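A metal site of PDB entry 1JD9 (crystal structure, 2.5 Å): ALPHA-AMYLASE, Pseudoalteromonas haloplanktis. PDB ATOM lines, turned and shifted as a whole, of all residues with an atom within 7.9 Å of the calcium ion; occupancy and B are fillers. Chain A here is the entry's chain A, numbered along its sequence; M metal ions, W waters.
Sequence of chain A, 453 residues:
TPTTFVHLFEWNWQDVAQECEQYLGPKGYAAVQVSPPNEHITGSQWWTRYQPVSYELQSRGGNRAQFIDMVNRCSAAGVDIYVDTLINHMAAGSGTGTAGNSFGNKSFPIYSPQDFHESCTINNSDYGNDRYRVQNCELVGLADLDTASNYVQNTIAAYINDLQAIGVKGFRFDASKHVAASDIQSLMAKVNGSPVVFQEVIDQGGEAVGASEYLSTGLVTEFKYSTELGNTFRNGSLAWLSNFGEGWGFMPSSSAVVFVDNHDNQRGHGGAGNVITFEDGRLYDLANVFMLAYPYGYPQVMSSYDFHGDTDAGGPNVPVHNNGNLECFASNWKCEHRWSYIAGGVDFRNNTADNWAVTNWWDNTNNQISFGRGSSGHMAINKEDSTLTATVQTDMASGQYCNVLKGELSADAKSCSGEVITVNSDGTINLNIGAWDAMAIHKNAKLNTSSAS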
ATOM      1  N   ILE A  87      -2.631  15.135 -36.030  1.00  0.00           N
ATOM      2  CA  ILE A  87      -2.864  13.706 -36.073  1.00  0.00           C
ATOM      3  C   ILE A  87      -3.879  13.184 -35.065  1.00  0.00           C
ATOM      4  O   ILE A  87      -4.398  12.075 -35.217  1.00  0.00           O
ATOM      5  CB  ILE A  87      -1.530  12.928 -35.901  1.00  0.00           C
ATOM      6  CG1 ILE A  87      -0.906  13.241 -34.541  1.00  0.00           C
ATOM      7  CG2 ILE A  87      -0.578  13.312 -37.029  1.00  0.00           C
ATOM      8  CD1 ILE A  87       0.216  12.307 -34.141  1.00  0.00           C
ATOM      9  N   ASN A  88      -4.204  13.985 -34.057  1.00  0.00           N
ATOM     10  CA  ASN A  88      -5.124  13.559 -33.019  1.00  0.00           C
ATOM     11  C   ASN A  88      -6.614  13.829 -33.274  1.00  0.00           C
ATOM     12  O   ASN A  88      -7.474  13.045 -32.848  1.00  0.00           O
ATOM     13  CB  ASN A  88      -4.716  14.216 -31.690  1.00  0.00           C
ATOM     14  CG  ASN A  88      -5.573  13.778 -30.502  1.00  0.00           C
ATOM     15  OD1 ASN A  88      -5.538  12.618 -30.088  1.00  0.00           O
ATOM     16  ND2 ASN A  88      -6.350  14.713 -29.958  1.00  0.00           N
ATOM     17  N   HIS A  89      -6.936  14.890 -34.008  1.00  0.00           N
ATOM     18  CA  HIS A  89      -8.327  15.256 -34.195  1.00  0.00           C
ATOM     19  C   HIS A  89      -8.693  15.980 -35.470  1.00  0.00           C
ATOM     20  O   HIS A  89      -7.876  16.145 -36.365  1.00  0.00           O
ATOM     21  CB  HIS A  89      -8.732  16.154 -33.031  1.00  0.00           C
ATOM     22  CG  HIS A  89      -7.834  17.329 -32.855  1.00  0.00           C
ATOM     23  ND1 HIS A  89      -6.653  17.269 -32.148  1.00  0.00           N
ATOM     24  CD2 HIS A  89      -7.915  18.594 -33.348  1.00  0.00           C
ATOM     25  CE1 HIS A  89      -6.037  18.444 -32.213  1.00  0.00           C
ATOM     26  NE2 HIS A  89      -6.785  19.259 -32.926  1.00  0.00           N
ATOM     27  N   HIS A 117     -13.455   8.308 -32.177  1.00  0.00           N
ATOM     28  CA  HIS A 117     -13.645   7.627 -30.912  1.00  0.00           C
ATOM     29  C   HIS A 117     -14.989   8.090 -30.367  1.00  0.00           C
ATOM     30  O   HIS A 117     -15.418   9.208 -30.664  1.00  0.00           O
ATOM     31  CB  HIS A 117     -12.531   8.024 -29.942  1.00  0.00           C
ATOM     32  CG  HIS A 117     -11.225   7.352 -30.226  1.00  0.00           C
ATOM     33  ND1 HIS A 117     -10.011   7.981 -30.050  1.00  0.00           N
ATOM     34  CD2 HIS A 117     -10.938   6.074 -30.567  1.00  0.00           C
ATOM     35  CE1 HIS A 117      -9.032   7.121 -30.267  1.00  0.00           C
ATOM     36  NE2 HIS A 117      -9.566   5.953 -30.587  1.00  0.00           N
ATOM     37  N   ILE A 122     -12.313  15.201 -22.012  1.00  0.00           N
ATOM     38  CA  ILE A 122     -11.065  15.045 -21.279  1.00  0.00           C
ATOM     39  C   ILE A 122     -11.105  16.022 -20.114  1.00  0.00           C
ATOM     40  O   ILE A 122     -11.342  17.196 -20.318  1.00  0.00           O
ATOM     41  CB  ILE A 122      -9.837  15.396 -22.143  1.00  0.00           C
ATOM     42  CG1 ILE A 122      -9.717  14.406 -23.301  1.00  0.00           C
ATOM     43  CG2 ILE A 122      -8.591  15.366 -21.277  1.00  0.00           C
ATOM     44  CD1 ILE A 122      -8.558  14.692 -24.214  1.00  0.00           C
ATOM     45  N   TYR A 132      -6.198   6.436 -20.569  1.00  0.00           N
ATOM     46  CA  TYR A 132      -7.281   6.061 -21.478  1.00  0.00           C
ATOM     47  C   TYR A 132      -8.076   7.295 -21.887  1.00  0.00           C
ATOM     48  O   TYR A 132      -8.216   7.562 -23.076  1.00  0.00           O
ATOM     49  CB  TYR A 132      -8.227   5.061 -20.816  1.00  0.00           C
ATOM     50  CG  TYR A 132      -9.427   4.714 -21.684  1.00  0.00           C
ATOM     51  CD1 TYR A 132      -9.349   3.686 -22.638  1.00  0.00           C
ATOM     52  CD2 TYR A 132     -10.607   5.455 -21.604  1.00  0.00           C
ATOM     53  CE1 TYR A 132     -10.432   3.422 -23.489  1.00  0.00           C
ATOM     54  CE2 TYR A 132     -11.691   5.196 -22.447  1.00  0.00           C
ATOM     55  CZ  TYR A 132     -11.595   4.178 -23.380  1.00  0.00           C
ATOM     56  OH  TYR A 132     -12.647   3.925 -24.223  1.00  0.00           O
ATOM     57  N   ARG A 133      -8.597   8.026 -20.903  1.00  0.00           N
ATOM     58  CA  ARG A 133      -9.397   9.230 -21.194  1.00  0.00           C
ATOM     59  C   ARG A 133      -8.626  10.335 -21.901  1.00  0.00           C
ATOM     60  O   ARG A 133      -9.194  11.108 -22.673  1.00  0.00           O
ATOM     61  CB  ARG A 133     -10.011   9.785 -19.917  1.00  0.00           C
ATOM     62  CG  ARG A 133     -11.139   8.954 -19.394  1.00  0.00           C
ATOM     63  CD  ARG A 133     -12.000   9.796 -18.503  1.00  0.00           C
ATOM     64  NE  ARG A 133     -13.401   9.662 -18.896  1.00  0.00           N
ATOM     65  CZ  ARG A 133     -14.247  10.683 -18.981  1.00  0.00           C
ATOM     66  NH1 ARG A 133     -13.819  11.906 -18.724  1.00  0.00           N
ATOM     67  NH2 ARG A 133     -15.506  10.471 -19.352  1.00  0.00           N
ATOM     68  N   VAL A 134      -7.324  10.409 -21.613  1.00  0.00           N
ATOM     69  CA  VAL A 134      -6.478  11.413 -22.229  1.00  0.00           C
ATOM     70  C   VAL A 134      -6.355  11.156 -23.734  1.00  0.00           C
ATOM     71  O   VAL A 134      -6.516  12.062 -24.536  1.00  0.00           O
ATOM     72  CB  VAL A 134      -5.055  11.416 -21.584  1.00  0.00           C
ATOM     73  CG1 VAL A 134      -4.095  12.297 -22.382  1.00  0.00           C
ATOM     74  CG2 VAL A 134      -5.131  11.922 -20.148  1.00  0.00           C
ATOM     75  N   GLN A 135      -6.108   9.910 -24.114  1.00  0.00           N
ATOM     76  CA  GLN A 135      -5.928   9.581 -25.525  1.00  0.00           C
ATOM     77  C   GLN A 135      -7.192   9.194 -26.289  1.00  0.00           C
ATOM     78  O   GLN A 135      -7.182   9.143 -27.522  1.00  0.00           O
ATOM     79  CB  GLN A 135      -4.862   8.491 -25.672  1.00  0.00           C
ATOM     80  CG  GLN A 135      -3.646   8.768 -24.814  1.00  0.00           C
ATOM     81  CD  GLN A 135      -2.574   7.714 -24.923  1.00  0.00           C
ATOM     82  OE1 GLN A 135      -2.869   6.519 -25.001  1.00  0.00           O
ATOM     83  NE2 GLN A 135      -1.308   8.154 -24.904  1.00  0.00           N
ATOM     84  N   ASN A 136      -8.289   8.940 -25.586  1.00  0.00           N
ATOM     85  CA  ASN A 136      -9.502   8.554 -26.295  1.00  0.00           C
ATOM     86  C   ASN A 136     -10.621   9.579 -26.281  1.00  0.00           C
ATOM     87  O   ASN A 136     -11.426   9.623 -27.201  1.00  0.00           O
ATOM     88  CB  ASN A 136     -10.023   7.213 -25.786  1.00  0.00           C
ATOM     89  CG  ASN A 136      -9.146   6.048 -26.220  1.00  0.00           C
ATOM     90  OD1 ASN A 136      -9.001   5.791 -27.405  1.00  0.00           O
ATOM     91  ND2 ASN A 136      -8.544   5.358 -25.258  1.00  0.00           N
ATOM     92  N   CYS A 137     -10.682  10.416 -25.242  1.00  0.00           N
ATOM     93  CA  CYS A 137     -11.732  11.428 -25.224  1.00  0.00           C
ATOM     94  C   CYS A 137     -11.344  12.652 -26.009  1.00  0.00           C
ATOM     95  O   CYS A 137     -10.203  12.777 -26.472  1.00  0.00           O
ATOM     96  CB  CYS A 137     -12.113  11.825 -23.797  1.00  0.00           C
ATOM     97  SG  CYS A 137     -12.790  10.411 -22.879  1.00  0.00           S
ATOM     98  N   GLU A 138     -12.302  13.561 -26.153  1.00  0.00           N
ATOM     99  CA  GLU A 138     -12.093  14.783 -26.910  1.00  0.00           C
ATOM    100  C   GLU A 138     -11.342  15.843 -26.110  1.00  0.00           C
ATOM    101  O   GLU A 138     -11.602  16.077 -24.924  1.00  0.00           O
ATOM    102  CB  GLU A 138     -13.441  15.329 -27.399  1.00  0.00           C
ATOM    103  CG  GLU A 138     -14.225  14.298 -28.222  1.00  0.00           C
ATOM    104  CD  GLU A 138     -15.645  14.726 -28.602  1.00  0.00           C
ATOM    105  OE1 GLU A 138     -16.451  15.019 -27.692  1.00  0.00           O
ATOM    106  OE2 GLU A 138     -15.948  14.761 -29.809  1.00  0.00           O
ATOM    107  N   LEU A 139     -10.369  16.461 -26.786  1.00  0.00           N
ATOM    108  CA  LEU A 139      -9.557  17.518 -26.210  1.00  0.00           C
ATOM    109  C   LEU A 139     -10.235  18.818 -26.553  1.00  0.00           C
ATOM    110  O   LEU A 139     -10.307  19.193 -27.723  1.00  0.00           O
ATOM    111  CB  LEU A 139      -8.159  17.490 -26.816  1.00  0.00           C
ATOM    112  CG  LEU A 139      -7.307  18.713 -26.472  1.00  0.00           C
ATOM    113  CD1 LEU A 139      -7.109  18.800 -24.970  1.00  0.00           C
ATOM    114  CD2 LEU A 139      -5.964  18.632 -27.195  1.00  0.00           C
ATOM    115  N   LEU A 142     -12.650  18.802 -29.553  1.00  0.00           N
ATOM    116  CA  LEU A 142     -12.223  18.401 -30.898  1.00  0.00           C
ATOM    117  C   LEU A 142     -12.526  16.929 -31.139  1.00  0.00           C
ATOM    118  O   LEU A 142     -12.168  16.087 -30.321  1.00  0.00           O
ATOM    119  CB  LEU A 142     -10.725  18.624 -31.092  1.00  0.00           C
ATOM    120  CG  LEU A 142     -10.279  20.067 -31.253  1.00  0.00           C
ATOM    121  CD1 LEU A 142     -11.026  20.693 -32.397  1.00  0.00           C
ATOM    122  CD2 LEU A 142     -10.547  20.817 -29.971  1.00  0.00           C
ATOM    123  N   ALA A 143     -13.163  16.614 -32.268  1.00  0.00           N
ATOM    124  CA  ALA A 143     -13.476  15.221 -32.578  1.00  0.00           C
ATOM    125  C   ALA A 143     -12.183  14.438 -32.518  1.00  0.00           C
ATOM    126  O   ALA A 143     -11.208  14.780 -33.186  1.00  0.00           O
ATOM    127  CB  ALA A 143     -14.076  15.107 -33.962  1.00  0.00           C
ATOM    128  N   ASP A 144     -12.151  13.380 -31.711  1.00  0.00           N
ATOM    129  CA  ASP A 144     -10.934  12.588 -31.580  1.00  0.00           C
ATOM    130  C   ASP A 144     -10.880  11.462 -32.616  1.00  0.00           C
ATOM    131  O   ASP A 144     -11.708  10.547 -32.597  1.00  0.00           O
ATOM    132  CB  ASP A 144     -10.866  12.013 -30.162  1.00  0.00           C
ATOM    133  CG  ASP A 144      -9.452  11.700 -29.740  1.00  0.00           C
ATOM    134  OD1 ASP A 144      -8.639  12.646 -29.661  1.00  0.00           O
ATOM    135  OD2 ASP A 144      -9.163  10.515 -29.499  1.00  0.00           O
ATOM    136  N   LEU A 145      -9.907  11.520 -33.528  1.00  0.00           N
ATOM    137  CA  LEU A 145      -9.782  10.499 -34.567  1.00  0.00           C
ATOM    138  C   LEU A 145      -9.396   9.162 -33.989  1.00  0.00           C
ATOM    139  O   LEU A 145      -8.705   9.071 -32.977  1.00  0.00           O
ATOM    140  CB  LEU A 145      -8.722  10.895 -35.604  1.00  0.00           C
ATOM    141  CG  LEU A 145      -9.040  11.895 -36.722  1.00  0.00           C
ATOM    142  CD1 LEU A 145      -7.764  12.247 -37.459  1.00  0.00           C
ATOM    143  CD2 LEU A 145     -10.061  11.310 -37.686  1.00  0.00           C
ATOM    144  N   ASP A 146      -9.853   8.110 -34.661  1.00  0.00           N
ATOM    145  CA  ASP A 146      -9.552   6.759 -34.242  1.00  0.00           C
ATOM    146  C   ASP A 146      -8.200   6.365 -34.846  1.00  0.00           C
ATOM    147  O   ASP A 146      -8.122   5.657 -35.850  1.00  0.00           O
ATOM    148  CB  ASP A 146     -10.661   5.825 -34.695  1.00  0.00           C
ATOM    149  CG  ASP A 146     -10.430   4.397 -34.269  1.00  0.00           C
ATOM    150  OD1 ASP A 146      -9.449   4.153 -33.519  1.00  0.00           O
ATOM    151  OD2 ASP A 146     -11.232   3.540 -34.689  1.00  0.00           O
ATOM    152  N   THR A 147      -7.141   6.829 -34.198  1.00  0.00           N
ATOM    153  CA  THR A 147      -5.781   6.593 -34.653  1.00  0.00           C
ATOM    154  C   THR A 147      -5.356   5.125 -34.737  1.00  0.00           C
ATOM    155  O   THR A 147      -4.252   4.827 -35.169  1.00  0.00           O
ATOM    156  CB  THR A 147      -4.818   7.384 -33.765  1.00  0.00           C
ATOM    157  OG1 THR A 147      -5.164   7.183 -32.398  1.00  0.00           O
ATOM    158  CG2 THR A 147      -4.919   8.857 -34.098  1.00  0.00           C
ATOM    159  N   ALA A 175      -0.245  17.621 -30.549  1.00  0.00           N
ATOM    160  CA  ALA A 175      -1.077  16.928 -29.573  1.00  0.00           C
ATOM    161  C   ALA A 175      -0.747  15.455 -29.531  1.00  0.00           C
ATOM    162  O   ALA A 175      -1.646  14.614 -29.424  1.00  0.00           O
ATOM    163  CB  ALA A 175      -2.559  17.139 -29.896  1.00  0.00           C
ATOM    164  N   SER A 176       0.532  15.125 -29.602  1.00  0.00           N
ATOM    165  CA  SER A 176       0.953  13.736 -29.570  1.00  0.00           C
ATOM    166  C   SER A 176       0.669  13.042 -28.246  1.00  0.00           C
ATOM    167  O   SER A 176       0.609  11.818 -28.178  1.00  0.00           O
ATOM    168  CB  SER A 176       2.451  13.628 -29.877  1.00  0.00           C
ATOM    169  OG  SER A 176       2.660  13.714 -31.279  1.00  0.00           O
ATOM    170  N   LYS A 177       0.484  13.815 -27.178  1.00  0.00           N
ATOM    171  CA  LYS A 177       0.195  13.202 -25.899  1.00  0.00           C
ATOM    172  C   LYS A 177      -1.178  12.569 -25.932  1.00  0.00           C
ATOM    173  O   LYS A 177      -1.467  11.612 -25.208  1.00  0.00           O
ATOM    174  CB  LYS A 177       0.251  14.234 -24.785  1.00  0.00           C
ATOM    175  CG  LYS A 177       0.011  13.638 -23.426  1.00  0.00           C
ATOM    176  CD  LYS A 177       0.370  14.604 -22.329  1.00  0.00           C
ATOM    177  CE  LYS A 177      -0.498  15.831 -22.351  1.00  0.00           C
ATOM    178  NZ  LYS A 177      -0.111  16.711 -21.227  1.00  0.00           N
ATOM    179  N   HIS A 178      -2.038  13.103 -26.793  1.00  0.00           N
ATOM    180  CA  HIS A 178      -3.394  12.607 -26.907  1.00  0.00           C
ATOM    181  C   HIS A 178      -3.543  11.464 -27.906  1.00  0.00           C
ATOM    182  O   HIS A 178      -4.646  11.106 -28.316  1.00  0.00           O
ATOM    183  CB  HIS A 178      -4.321  13.770 -27.246  1.00  0.00           C
ATOM    184  CG  HIS A 178      -4.364  14.834 -26.190  1.00  0.00           C
ATOM    185  ND1 HIS A 178      -3.321  15.707 -25.960  1.00  0.00           N
ATOM    186  CD2 HIS A 178      -5.313  15.141 -25.271  1.00  0.00           C
ATOM    187  CE1 HIS A 178      -3.624  16.515 -24.954  1.00  0.00           C
ATOM    188  NE2 HIS A 178      -4.840  16.191 -24.523  1.00  0.00           N
ATOM    189  N   VAL A 179      -2.414  10.888 -28.289  1.00  0.00           N
ATOM    190  CA  VAL A 179      -2.389   9.778 -29.218  1.00  0.00           C
ATOM    191  C   VAL A 179      -1.408   8.732 -28.720  1.00  0.00           C
ATOM    192  O   VAL A 179      -0.230   9.025 -28.476  1.00  0.00           O
ATOM    193  CB  VAL A 179      -1.972  10.201 -30.631  1.00  0.00           C
ATOM    194  CG1 VAL A 179      -2.073   9.003 -31.587  1.00  0.00           C
ATOM    195  CG2 VAL A 179      -2.836  11.336 -31.102  1.00  0.00           C
ATOM    196  N   ALA A 180      -1.911   7.527 -28.572  1.00  0.00           N
ATOM    197  CA  ALA A 180      -1.117   6.396 -28.099  1.00  0.00           C
ATOM    198  C   ALA A 180       0.149   6.242 -28.940  1.00  0.00           C
ATOM    199  O   ALA A 180       0.093   6.238 -30.178  1.00  0.00           O
ATOM    200  CB  ALA A 180      -1.950   5.133 -28.183  1.00  0.00           C
ATOM    201  N   ASP A 183      -0.023   3.806 -31.749  1.00  0.00           N
ATOM    202  CA  ASP A 183      -0.673   4.273 -32.954  1.00  0.00           C
ATOM    203  C   ASP A 183       0.316   5.079 -33.782  1.00  0.00           C
ATOM    204  O   ASP A 183       0.284   5.035 -35.001  1.00  0.00           O
ATOM    205  CB  ASP A 183      -1.876   5.152 -32.618  1.00  0.00           C
ATOM    206  CG  ASP A 183      -2.965   4.387 -31.891  1.00  0.00           C
ATOM    207  OD1 ASP A 183      -3.800   5.057 -31.232  1.00  0.00           O
ATOM    208  OD2 ASP A 183      -2.993   3.147 -32.003  1.00  0.00           O
HETATM  209 CA    CA M   1      -6.854  11.007 -29.183  1.00  0.00          CA
HETATM  210  O   HOH W   1      -7.789  12.455 -27.035  1.00  0.00           O
HETATM  211  O   HOH W   2      -6.764  10.725 -31.676  1.00  0.00           O
HETATM  212  O   HOH W   3      -6.056   8.864 -29.868  1.00  0.00           O
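The backbone carbonyl oxygen of Asp 144 sits at hydrogen-bond distance from the backbone NH of His 117 (2.9 Å).
A ring nitrogen (ND1) of His 89 is in hydrogen-bond range of the side-chain amide nitrogen of Asn 88, at 3.4 Å.
O of Asn 88 lies within hydrogen-bond range of N of Leu 145 (3.0 Å).
The backbone carbonyl oxygen (O) of Lys 177 lies within hydrogen-bond range of the side-chain amide nitrogen (NE2) of Gln 135, 3.5 Å away.
Water W2 lies within hydrogen-bond range of O of Asn 88 (2.7 Å) and O of Leu 145 (2.9 Å).
The calcium ion is bound by OD1 of Asn 88 (2.3 Å), O of His 178 (2.4 Å), OD2 of Asp 144 (2.4 Å), water W3 (2.4 Å), OD1 of Asp 144 (2.5 Å), water W2 (2.5 Å), O of Gln 135 (2.5 Å) and water W1 (2.8 Å).
Within 4 Å of the calcium ion: Asn 88, Gln 135, Asp 144 and His 178.
The nearest printed residue that does not touch the calcium ion is Asn 136 (4.4 Å).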
